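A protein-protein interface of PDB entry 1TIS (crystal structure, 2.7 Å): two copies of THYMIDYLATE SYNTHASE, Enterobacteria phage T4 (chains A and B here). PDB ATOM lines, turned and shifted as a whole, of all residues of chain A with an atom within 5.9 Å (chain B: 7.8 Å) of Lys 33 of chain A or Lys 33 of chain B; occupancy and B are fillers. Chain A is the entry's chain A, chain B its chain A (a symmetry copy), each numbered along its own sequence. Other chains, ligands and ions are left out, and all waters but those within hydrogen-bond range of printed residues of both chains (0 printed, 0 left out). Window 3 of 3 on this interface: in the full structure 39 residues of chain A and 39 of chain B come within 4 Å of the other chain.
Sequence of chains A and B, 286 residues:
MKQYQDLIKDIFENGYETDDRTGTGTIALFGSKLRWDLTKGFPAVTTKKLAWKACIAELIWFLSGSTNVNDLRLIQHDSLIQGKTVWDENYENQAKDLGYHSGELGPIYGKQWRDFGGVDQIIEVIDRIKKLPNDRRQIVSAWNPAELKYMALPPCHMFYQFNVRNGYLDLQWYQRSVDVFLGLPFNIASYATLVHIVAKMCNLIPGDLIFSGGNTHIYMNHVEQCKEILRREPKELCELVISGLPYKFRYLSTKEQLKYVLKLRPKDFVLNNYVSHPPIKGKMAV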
ATOM      1  N   GLY A  31      12.523  15.784   4.357  1.00  0.00           N
ATOM      2  CA  GLY A  31      12.142  14.610   5.090  1.00  0.00           C
ATOM      3  C   GLY A  31      12.503  14.755   6.520  1.00  0.00           C
ATOM      4  O   GLY A  31      13.412  14.085   6.940  1.00  0.00           O
ATOM      5  N   SER A  32      11.872  15.564   7.348  1.00  0.00           N
ATOM      6  CA  SER A  32      12.224  15.652   8.766  1.00  0.00           C
ATOM      7  C   SER A  32      11.034  15.192   9.618  1.00  0.00           C
ATOM      8  O   SER A  32       9.945  15.010   9.094  1.00  0.00           O
ATOM      9  CB  SER A  32      12.600  17.097   9.051  1.00  0.00           C
ATOM     10  OG  SER A  32      13.277  17.578   7.892  1.00  0.00           O
ATOM     11  N   LYS A  33      11.142  14.963  10.917  1.00  0.00           N
ATOM     12  CA  LYS A  33      10.049  14.620  11.819  1.00  0.00           C
ATOM     13  C   LYS A  33      10.609  14.899  13.218  1.00  0.00           C
ATOM     14  O   LYS A  33      11.820  14.781  13.438  1.00  0.00           O
ATOM     15  CB  LYS A  33       9.682  13.159  11.632  1.00  0.00           C
ATOM     16  CG  LYS A  33       8.851  12.527  12.737  1.00  0.00           C
ATOM     17  CD  LYS A  33       8.115  11.279  12.234  1.00  0.00           C
ATOM     18  CE  LYS A  33       7.008  11.788  11.315  1.00  0.00           C
ATOM     19  NZ  LYS A  33       6.290  10.742  10.624  1.00  0.00           N
ATOM     20  N   LEU A  34       9.848  15.369  14.182  1.00  0.00           N
ATOM     21  CA  LEU A  34      10.361  15.590  15.532  1.00  0.00           C
ATOM     22  C   LEU A  34       9.239  15.123  16.466  1.00  0.00           C
ATOM     23  O   LEU A  34       8.150  14.901  15.929  1.00  0.00           O
ATOM     24  CB  LEU A  34      10.616  17.067  15.768  1.00  0.00           C
ATOM     25  CG  LEU A  34      11.481  17.887  14.822  1.00  0.00           C
ATOM     26  CD1 LEU A  34      11.433  19.315  15.307  1.00  0.00           C
ATOM     27  CD2 LEU A  34      12.929  17.424  14.795  1.00  0.00           C
ATOM     28  N   ARG A  35       9.344  14.933  17.791  1.00  0.00           N
ATOM     29  CA  ARG A  35       8.180  14.598  18.610  1.00  0.00           C
ATOM     30  C   ARG A  35       8.284  15.382  19.900  1.00  0.00           C
ATOM     31  O   ARG A  35       9.379  15.459  20.453  1.00  0.00           O
ATOM     32  CB  ARG A  35       8.107  13.086  18.909  1.00  0.00           C
ATOM     33  CG  ARG A  35       9.402  12.386  19.260  1.00  0.00           C
ATOM     34  CD  ARG A  35      10.366  11.930  18.133  1.00  0.00           C
ATOM     35  NE  ARG A  35      11.653  11.579  18.744  1.00  0.00           N
ATOM     36  CZ  ARG A  35      12.844  11.900  18.200  1.00  0.00           C
ATOM     37  NH1 ARG A  35      12.946  12.468  16.987  1.00  0.00           N
ATOM     38  NH2 ARG A  35      13.976  11.622  18.867  1.00  0.00           N
ATOM     39  N   GLN A 172      -0.375  15.331  14.629  1.00  0.00           N
ATOM     40  CA  GLN A 172       0.798  15.331  13.756  1.00  0.00           C
ATOM     41  C   GLN A 172       0.531  16.078  12.443  1.00  0.00           C
ATOM     42  O   GLN A 172      -0.350  15.713  11.682  1.00  0.00           O
ATOM     43  CB  GLN A 172       1.214  13.876  13.470  1.00  0.00           C
ATOM     44  CG  GLN A 172       2.203  13.820  12.344  1.00  0.00           C
ATOM     45  CD  GLN A 172       2.702  12.441  12.112  1.00  0.00           C
ATOM     46  OE1 GLN A 172       3.909  12.279  12.128  1.00  0.00           O
ATOM     47  NE2 GLN A 172       1.909  11.403  11.942  1.00  0.00           N
ATOM     48  N   TYR A 174       1.692  17.655   8.604  1.00  0.00           N
ATOM     49  CA  TYR A 174       2.675  17.503   7.534  1.00  0.00           C
ATOM     50  C   TYR A 174       2.808  18.906   6.933  1.00  0.00           C
ATOM     51  O   TYR A 174       1.804  19.604   6.744  1.00  0.00           O
ATOM     52  CB  TYR A 174       2.173  16.500   6.527  1.00  0.00           C
ATOM     53  CG  TYR A 174       3.164  16.214   5.438  1.00  0.00           C
ATOM     54  CD1 TYR A 174       3.380  17.143   4.427  1.00  0.00           C
ATOM     55  CD2 TYR A 174       3.824  15.011   5.474  1.00  0.00           C
ATOM     56  CE1 TYR A 174       4.281  16.864   3.426  1.00  0.00           C
ATOM     57  CE2 TYR A 174       4.717  14.722   4.468  1.00  0.00           C
ATOM     58  CZ  TYR A 174       4.924  15.650   3.470  1.00  0.00           C
ATOM     59  OH  TYR A 174       5.786  15.336   2.471  1.00  0.00           O
ATOM     60  N   ILE A 210       3.857  15.726  17.023  1.00  0.00           N
ATOM     61  CA  ILE A 210       4.829  15.190  16.067  1.00  0.00           C
ATOM     62  C   ILE A 210       4.747  16.001  14.812  1.00  0.00           C
ATOM     63  O   ILE A 210       3.662  16.407  14.442  1.00  0.00           O
ATOM     64  CB  ILE A 210       4.508  13.752  15.715  1.00  0.00           C
ATOM     65  CG1 ILE A 210       4.181  12.924  16.927  1.00  0.00           C
ATOM     66  CG2 ILE A 210       5.727  13.133  15.097  1.00  0.00           C
ATOM     67  CD1 ILE A 210       3.605  11.589  16.424  1.00  0.00           C
ATOM     68  N   PHE A 211       5.803  16.217  14.064  1.00  0.00           N
ATOM     69  CA  PHE A 211       5.763  17.095  12.897  1.00  0.00           C
ATOM     70  C   PHE A 211       6.459  16.401  11.750  1.00  0.00           C
ATOM     71  O   PHE A 211       7.626  16.030  11.966  1.00  0.00           O
ATOM     72  CB  PHE A 211       6.484  18.431  13.206  1.00  0.00           C
ATOM     73  CG  PHE A 211       7.188  19.125  12.044  1.00  0.00           C
ATOM     74  CD1 PHE A 211       6.476  19.779  11.063  1.00  0.00           C
ATOM     75  CD2 PHE A 211       8.561  19.085  11.970  1.00  0.00           C
ATOM     76  CE1 PHE A 211       7.135  20.387  10.011  1.00  0.00           C
ATOM     77  CE2 PHE A 211       9.218  19.690  10.920  1.00  0.00           C
ATOM     78  CZ  PHE A 211       8.507  20.347   9.936  1.00  0.00           C
ATOM     79  N   SER A 212       5.811  16.306  10.577  1.00  0.00           N
ATOM     80  CA  SER A 212       6.460  15.663   9.458  1.00  0.00           C
ATOM     81  C   SER A 212       6.862  16.742   8.477  1.00  0.00           C
ATOM     82  O   SER A 212       6.082  17.651   8.158  1.00  0.00           O
ATOM     83  CB  SER A 212       5.504  14.686   8.855  1.00  0.00           C
ATOM     84  OG  SER A 212       5.032  13.750   9.820  1.00  0.00           O
ATOM     85  N   GLY A 213       8.069  16.677   7.956  1.00  0.00           N
ATOM     86  CA  GLY A 213       8.546  17.744   7.106  1.00  0.00           C
ATOM     87  C   GLY A 213       8.795  17.283   5.690  1.00  0.00           C
ATOM     88  O   GLY A 213       9.137  16.124   5.405  1.00  0.00           O
ATOM     89  N   GLN B   3      17.189  -0.213   8.471  1.00  0.00           N
ATOM     90  CA  GLN B   3      16.197   0.447   9.291  1.00  0.00           C
ATOM     91  C   GLN B   3      14.867  -0.245   9.434  1.00  0.00           C
ATOM     92  O   GLN B   3      14.124   0.131  10.335  1.00  0.00           O
ATOM     93  CB  GLN B   3      15.969   1.899   8.781  1.00  0.00           C
ATOM     94  CG  GLN B   3      15.369   2.227   7.406  1.00  0.00           C
ATOM     95  CD  GLN B   3      16.142   1.691   6.204  1.00  0.00           C
ATOM     96  OE1 GLN B   3      16.222   0.472   5.979  1.00  0.00           O
ATOM     97  NE2 GLN B   3      16.778   2.534   5.402  1.00  0.00           N
ATOM     98  N   LEU B   7      12.771  -0.536  13.447  1.00  0.00           N
ATOM     99  CA  LEU B   7      11.441  -0.057  13.794  1.00  0.00           C
ATOM    100  C   LEU B   7      10.620  -1.062  14.555  1.00  0.00           C
ATOM    101  O   LEU B   7      10.184  -0.756  15.664  1.00  0.00           O
ATOM    102  CB  LEU B   7      10.614   0.352  12.558  1.00  0.00           C
ATOM    103  CG  LEU B   7       9.169   0.902  12.773  1.00  0.00           C
ATOM    104  CD1 LEU B   7       9.201   2.073  13.767  1.00  0.00           C
ATOM    105  CD2 LEU B   7       8.566   1.352  11.438  1.00  0.00           C
ATOM    106  N   PHE B  30       2.466   5.635  17.326  1.00  0.00           N
ATOM    107  CA  PHE B  30       2.021   6.685  16.386  1.00  0.00           C
ATOM    108  C   PHE B  30       3.145   7.648  16.010  1.00  0.00           C
ATOM    109  O   PHE B  30       3.666   8.370  16.867  1.00  0.00           O
ATOM    110  CB  PHE B  30       0.853   7.491  17.021  1.00  0.00           C
ATOM    111  CG  PHE B  30       0.358   8.726  16.274  1.00  0.00           C
ATOM    112  CD1 PHE B  30      -0.324   8.593  15.073  1.00  0.00           C
ATOM    113  CD2 PHE B  30       0.592   9.989  16.822  1.00  0.00           C
ATOM    114  CE1 PHE B  30      -0.764   9.725  14.426  1.00  0.00           C
ATOM    115  CE2 PHE B  30       0.145  11.118  16.168  1.00  0.00           C
ATOM    116  CZ  PHE B  30      -0.532  10.976  14.970  1.00  0.00           C
ATOM    117  N   GLY B  31       3.569   7.687  14.774  1.00  0.00           N
ATOM    118  CA  GLY B  31       4.545   8.674  14.407  1.00  0.00           C
ATOM    119  C   GLY B  31       5.801   8.019  13.970  1.00  0.00           C
ATOM    120  O   GLY B  31       6.758   8.101  14.697  1.00  0.00           O
ATOM    121  N   SER B  32       5.921   7.371  12.828  1.00  0.00           N
ATOM    122  CA  SER B  32       7.188   6.773  12.405  1.00  0.00           C
ATOM    123  C   SER B  32       7.673   7.455  11.120  1.00  0.00           C
ATOM    124  O   SER B  32       6.929   8.215  10.518  1.00  0.00           O
ATOM    125  CB  SER B  32       6.942   5.287  12.201  1.00  0.00           C
ATOM    126  OG  SER B  32       6.012   4.885  13.204  1.00  0.00           O
ATOM    127  N   LYS B  33       8.889   7.267  10.635  1.00  0.00           N
ATOM    128  CA  LYS B  33       9.400   7.793   9.376  1.00  0.00           C
ATOM    129  C   LYS B  33      10.643   6.946   9.085  1.00  0.00           C
ATOM    130  O   LYS B  33      11.305   6.474  10.016  1.00  0.00           O
ATOM    131  CB  LYS B  33       9.738   9.263   9.544  1.00  0.00           C
ATOM    132  CG  LYS B  33      10.632   9.875   8.478  1.00  0.00           C
ATOM    133  CD  LYS B  33      10.487  11.402   8.440  1.00  0.00           C
ATOM    134  CE  LYS B  33       9.112  11.675   7.833  1.00  0.00           C
ATOM    135  NZ  LYS B  33       8.729  13.067   7.848  1.00  0.00           N
ATOM    136  N   LEU B  34      10.976   6.611   7.857  1.00  0.00           N
ATOM    137  CA  LEU B  34      12.186   5.847   7.566  1.00  0.00           C
ATOM    138  C   LEU B  34      12.766   6.484   6.299  1.00  0.00           C
ATOM    139  O   LEU B  34      12.028   7.283   5.713  1.00  0.00           O
ATOM    140  CB  LEU B  34      11.843   4.398   7.276  1.00  0.00           C
ATOM    141  CG  LEU B  34      11.012   3.567   8.243  1.00  0.00           C
ATOM    142  CD1 LEU B  34      10.789   2.225   7.592  1.00  0.00           C
ATOM    143  CD2 LEU B  34      11.700   3.357   9.583  1.00  0.00           C
ATOM    144  N   ARG B  35      13.987   6.257   5.789  1.00  0.00           N
ATOM    145  CA  ARG B  35      14.400   6.829   4.508  1.00  0.00           C
ATOM    146  C   ARG B  35      15.175   5.767   3.760  1.00  0.00           C
ATOM    147  O   ARG B  35      15.990   5.088   4.380  1.00  0.00           O
ATOM    148  CB  ARG B  35      15.268   8.091   4.698  1.00  0.00           C
ATOM    149  CG  ARG B  35      16.317   8.051   5.788  1.00  0.00           C
ATOM    150  CD  ARG B  35      15.914   8.330   7.261  1.00  0.00           C
ATOM    151  NE  ARG B  35      17.028   7.924   8.125  1.00  0.00           N
ATOM    152  CZ  ARG B  35      16.860   7.281   9.298  1.00  0.00           C
ATOM    153  NH1 ARG B  35      15.644   7.064   9.827  1.00  0.00           N
ATOM    154  NH2 ARG B  35      17.935   6.864   9.987  1.00  0.00           N
ATOM    155  N   TRP B  36      14.972   5.552   2.462  1.00  0.00           N
ATOM    156  CA  TRP B  36      15.632   4.501   1.684  1.00  0.00           C
ATOM    157  C   TRP B  36      16.404   5.087   0.531  1.00  0.00           C
ATOM    158  O   TRP B  36      15.873   5.966  -0.141  1.00  0.00           O
ATOM    159  CB  TRP B  36      14.670   3.496   1.009  1.00  0.00           C
ATOM    160  CG  TRP B  36      13.872   2.618   1.941  1.00  0.00           C
ATOM    161  CD1 TRP B  36      14.373   1.441   2.407  1.00  0.00           C
ATOM    162  CD2 TRP B  36      12.654   2.948   2.446  1.00  0.00           C
ATOM    163  NE1 TRP B  36      13.466   1.021   3.240  1.00  0.00           N
ATOM    164  CE2 TRP B  36      12.425   1.883   3.299  1.00  0.00           C
ATOM    165  CE3 TRP B  36      11.735   3.968   2.329  1.00  0.00           C
ATOM    166  CZ2 TRP B  36      11.253   1.844   4.050  1.00  0.00           C
ATOM    167  CZ3 TRP B  36      10.580   3.920   3.079  1.00  0.00           C
ATOM    168  CH2 TRP B  36      10.338   2.868   3.935  1.00  0.00           C
ATOM    169  N   GLN B 172       7.745  10.889  -0.860  1.00  0.00           N
ATOM    170  CA  GLN B 172       7.434  10.617   0.544  1.00  0.00           C
ATOM    171  C   GLN B 172       5.928  10.429   0.767  1.00  0.00           C
ATOM    172  O   GLN B 172       5.138  11.321   0.501  1.00  0.00           O
ATOM    173  CB  GLN B 172       7.964  11.774   1.411  1.00  0.00           C
ATOM    174  CG  GLN B 172       7.401  11.696   2.799  1.00  0.00           C
ATOM    175  CD  GLN B 172       7.973  12.737   3.689  1.00  0.00           C
ATOM    176  OE1 GLN B 172       8.482  12.358   4.728  1.00  0.00           O
ATOM    177  NE2 GLN B 172       7.994  14.019   3.384  1.00  0.00           N
ATOM    178  N   TRP B 173       5.486   9.329   1.303  1.00  0.00           N
ATOM    179  CA  TRP B 173       4.075   9.096   1.526  1.00  0.00           C
ATOM    180  C   TRP B 173       3.742   9.294   2.971  1.00  0.00           C
ATOM    181  O   TRP B 173       4.620   9.245   3.861  1.00  0.00           O
ATOM    182  CB  TRP B 173       3.615   7.658   1.126  1.00  0.00           C
ATOM    183  CG  TRP B 173       4.625   6.523   1.194  1.00  0.00           C
ATOM    184  CD1 TRP B 173       5.918   6.561   0.687  1.00  0.00           C
ATOM    185  CD2 TRP B 173       4.385   5.358   1.818  1.00  0.00           C
ATOM    186  NE1 TRP B 173       6.501   5.429   1.013  1.00  0.00           N
ATOM    187  CE2 TRP B 173       5.612   4.692   1.688  1.00  0.00           C
ATOM    188  CE3 TRP B 173       3.301   4.841   2.458  1.00  0.00           C
ATOM    189  CZ2 TRP B 173       5.813   3.448   2.213  1.00  0.00           C
ATOM    190  CZ3 TRP B 173       3.498   3.588   2.989  1.00  0.00           C
ATOM    191  CH2 TRP B 173       4.725   2.910   2.872  1.00  0.00           C
ATOM    192  N   TYR B 174       2.471   9.576   3.195  1.00  0.00           N
ATOM    193  CA  TYR B 174       1.993   9.569   4.575  1.00  0.00           C
ATOM    194  C   TYR B 174       0.942   8.455   4.612  1.00  0.00           C
ATOM    195  O   TYR B 174       0.131   8.329   3.685  1.00  0.00           O
ATOM    196  CB  TYR B 174       1.406  10.914   4.912  1.00  0.00           C
ATOM    197  CG  TYR B 174       0.972  11.025   6.344  1.00  0.00           C
ATOM    198  CD1 TYR B 174      -0.189  10.394   6.773  1.00  0.00           C
ATOM    199  CD2 TYR B 174       1.749  11.775   7.191  1.00  0.00           C
ATOM    200  CE1 TYR B 174      -0.585  10.514   8.086  1.00  0.00           C
ATOM    201  CE2 TYR B 174       1.351  11.908   8.501  1.00  0.00           C
ATOM    202  CZ  TYR B 174       0.197  11.278   8.918  1.00  0.00           C
ATOM    203  OH  TYR B 174      -0.195  11.445  10.205  1.00  0.00           O
ATOM    204  N   LEU B 209      13.606   7.339  -0.800  1.00  0.00           N
ATOM    205  CA  LEU B 209      12.212   7.016  -0.542  1.00  0.00           C
ATOM    206  C   LEU B 209      11.975   7.242   0.928  1.00  0.00           C
ATOM    207  O   LEU B 209      12.661   6.575   1.686  1.00  0.00           O
ATOM    208  CB  LEU B 209      11.943   5.568  -0.910  1.00  0.00           C
ATOM    209  CG  LEU B 209      10.525   5.079  -0.894  1.00  0.00           C
ATOM    210  CD1 LEU B 209       9.678   5.751  -1.966  1.00  0.00           C
ATOM    211  CD2 LEU B 209      10.567   3.572  -1.107  1.00  0.00           C
ATOM    212  N   ILE B 210      11.067   8.113   1.390  1.00  0.00           N
ATOM    213  CA  ILE B 210      10.844   8.413   2.806  1.00  0.00           C
ATOM    214  C   ILE B 210       9.424   8.075   3.138  1.00  0.00           C
ATOM    215  O   ILE B 210       8.559   8.284   2.309  1.00  0.00           O
ATOM    216  CB  ILE B 210      11.051   9.887   3.089  1.00  0.00           C
ATOM    217  CG1 ILE B 210      12.298  10.426   2.442  1.00  0.00           C
ATOM    218  CG2 ILE B 210      11.232  10.065   4.567  1.00  0.00           C
ATOM    219  CD1 ILE B 210      12.245  11.959   2.557  1.00  0.00           C
ATOM    220  N   PHE B 211       9.084   7.634   4.326  1.00  0.00           N
ATOM    221  CA  PHE B 211       7.724   7.197   4.633  1.00  0.00           C
ATOM    222  C   PHE B 211       7.312   7.802   5.954  1.00  0.00           C
ATOM    223  O   PHE B 211       8.063   7.569   6.917  1.00  0.00           O
ATOM    224  CB  PHE B 211       7.666   5.653   4.731  1.00  0.00           C
ATOM    225  CG  PHE B 211       6.652   5.056   5.703  1.00  0.00           C
ATOM    226  CD1 PHE B 211       5.305   5.051   5.418  1.00  0.00           C
ATOM    227  CD2 PHE B 211       7.093   4.524   6.892  1.00  0.00           C
ATOM    228  CE1 PHE B 211       4.403   4.519   6.320  1.00  0.00           C
ATOM    229  CE2 PHE B 211       6.194   3.995   7.793  1.00  0.00           C
ATOM    230  CZ  PHE B 211       4.843   3.988   7.509  1.00  0.00           C
ATOM    231  N   SER B 212       6.147   8.468   6.013  1.00  0.00           N
ATOM    232  CA  SER B 212       5.719   9.041   7.268  1.00  0.00           C
ATOM    233  C   SER B 212       4.584   8.194   7.799  1.00  0.00           C
ATOM    234  O   SER B 212       3.656   7.823   7.067  1.00  0.00           O
ATOM    235  CB  SER B 212       5.296  10.453   7.023  1.00  0.00           C
ATOM    236  OG  SER B 212       6.331  11.212   6.405  1.00  0.00           O
ATOM    237  N   GLY B 213       4.607   7.870   9.075  1.00  0.00           N
ATOM    238  CA  GLY B 213       3.612   6.967   9.607  1.00  0.00           C
ATOM    239  C   GLY B 213       2.719   7.632  10.627  1.00  0.00           C
ATOM    240  O   GLY B 213       3.097   8.563  11.354  1.00  0.00           O
ATOM    241  N   GLY B 214       1.512   7.113  10.567  1.00  0.00           N
ATOM    242  CA  GLY B 214       0.534   7.478  11.539  1.00  0.00           C
ATOM    243  C   GLY B 214       0.448   6.334  12.532  1.00  0.00           C
ATOM    244  O   GLY B 214       1.377   6.078  13.314  1.00  0.00           O
ATOM    245  N   THR B 216       1.239   3.121  13.164  1.00  0.00           N
ATOM    246  CA  THR B 216       2.074   1.941  12.898  1.00  0.00           C
ATOM    247  C   THR B 216       1.770   0.906  13.998  1.00  0.00           C
ATOM    248  O   THR B 216       1.950   1.082  15.209  1.00  0.00           O
ATOM    249  CB  THR B 216       3.558   2.377  12.916  1.00  0.00           C
ATOM    250  OG1 THR B 216       3.755   3.222  11.781  1.00  0.00           O
ATOM    251  CG2 THR B 216       4.517   1.221  12.851  1.00  0.00           C
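Hydrophobic or aromatic side chains of chain A within 4 Å of the printed part of chain B: Tyr 174 and Ile 210. Along chain B the printed residues that touch a printed residue of chain A span positions 30 to 213. Among the printed residues, no Asp or Glu carboxylate lies within 4 Å of a Lys or Arg side-chain nitrogen of the other chain.
Lys 33 of chain A touches just these residues of chain B: Ser 32, Lys 33, Ser 212 and Gly 213. Lys 33 of chain B touches just these residues of chain A: Ser 32 (2.6 Å), Lys 33 (3.7 Å), Ser 212 (3.7 Å) and Gly 213 (3.7 Å). Printed residues of chain A within 4 Å of Ile 210 of chain B: Gly 31 (3.7 Å). Of the printed residues of chain B, Ile 210 of chain A touches Phe 30 and Gly 31. Of the printed residues of chain B, Gly 213 of chain A touches Lys 33 (3.7 Å) and Gln 172 (3.1 Å). Printed residues of chain A within 4 Å of Gln 172 of chain B: Tyr 174 (2.7 Å) and Gly 213 (3.1 Å). Of the printed residues of chain B, Ser 212 of chain A touches Lys 33 (3.7 Å). The nearest residue of chain B that does not touch Lys 33 of chain A is Gly 31 of chain B (4.2 Å).
Among the printed residues, pairs that only touch across the chains: Ile 210 of chain A with Phe 30 of chain B (3.2 Å), Ile 210 of chain A with Gly 31 of chain B (3.7 Å), Gly 31 of chain A with Ile 210 of chain B (3.7 Å), Gly 213 of chain A with Lys 33 of chain B (3.7 Å), Lys 33 of chain A with Gly 213 of chain B (3.7 Å), Gln 172 of chain A with Phe 30 of chain B (3.7 Å), Lys 33 of chain A with Lys 33 of chain B (3.7 Å), Ser 212 of chain A with Lys 33 of chain B (3.7 Å) and Lys 33 of chain A with Ser 212 of chain B (3.7 Å).
NZ of Lys 33 of chain B sits at hydrogen-bond distance from O of Ser 32 of chain A (2.6 Å). The backbone carbonyl oxygen (O) of Ser 32 of chain B lies within hydrogen-bond range of the side-chain amino group (NZ) of Lys 33 of chain A. The side-chain hydroxyl (OH) of Tyr 174 of chain B is in hydrogen-bond range of the side-chain amide nitrogen (NE2) of Gln 172 of chain A, 2.7 Å away. O of Gly 213 of chain B lies within hydrogen-bond range of NE2 of Gln 172 of chain A. NE2 of Gln 172 of chain B lies within hydrogen-bond range of OH of Tyr 174 of chain A. The backbone carbonyl oxygen (O) of Gly 213 of chain A sits at hydrogen-bond distance from the side-chain amide nitrogen (NE2) of Gln 172 of chain B, 3.1 Å away.
OG of Ser 212 of chain A lies close to NZ of Lys 33 of chain A. The side-chain amide oxygen (OE1) of Gln 172 of chain A lies within hydrogen-bond range of the side-chain hydroxyl (OG) of Ser 212 of chain A (3.0 Å). The backbone NH (N) of Gly 31 of chain B sits at hydrogen-bond distance from the backbone carbonyl oxygen (O) of Gly 214 of chain B, 3.1 Å away. The side-chain amino group of Lys 33 of chain B sits at hydrogen-bond distance from the side-chain amide oxygen of Gln 172 of chain B. The backbone NH (N) of Trp 173 of chain B is in hydrogen-bond range of the backbone carbonyl oxygen (O) of Ile 210 of chain B (3.4 Å). The backbone NH (N) of Ser 212 of chain B lies within hydrogen-bond range of the backbone carbonyl oxygen (O) of Trp 173 of chain B, 2.8 Å away.
Gly 31 of chain A touches Ile 210 of chain B, and with the chains exchanged Ile 210 of chain A touches Gly 31 of chain B. Ser 32 of chain A touches Lys 33 of chain B, and with the chains exchanged Lys 33 of chain A touches Ser 32 of chain B. Gln 172 of chain A touches Tyr 174 of chain B, and with the chains exchanged Tyr 174 of chain A touches Gln 172 of chain B. Gln 172 of chain A touches Gly 213 of chain B, and with the chains exchanged Gly 213 of chain A touches Gln 172 of chain B. 11 positions are printed for both chains. Of the 15 pairs that touch across the chains among the printed residues, 13 have their exchanged pair printed and touching as well.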
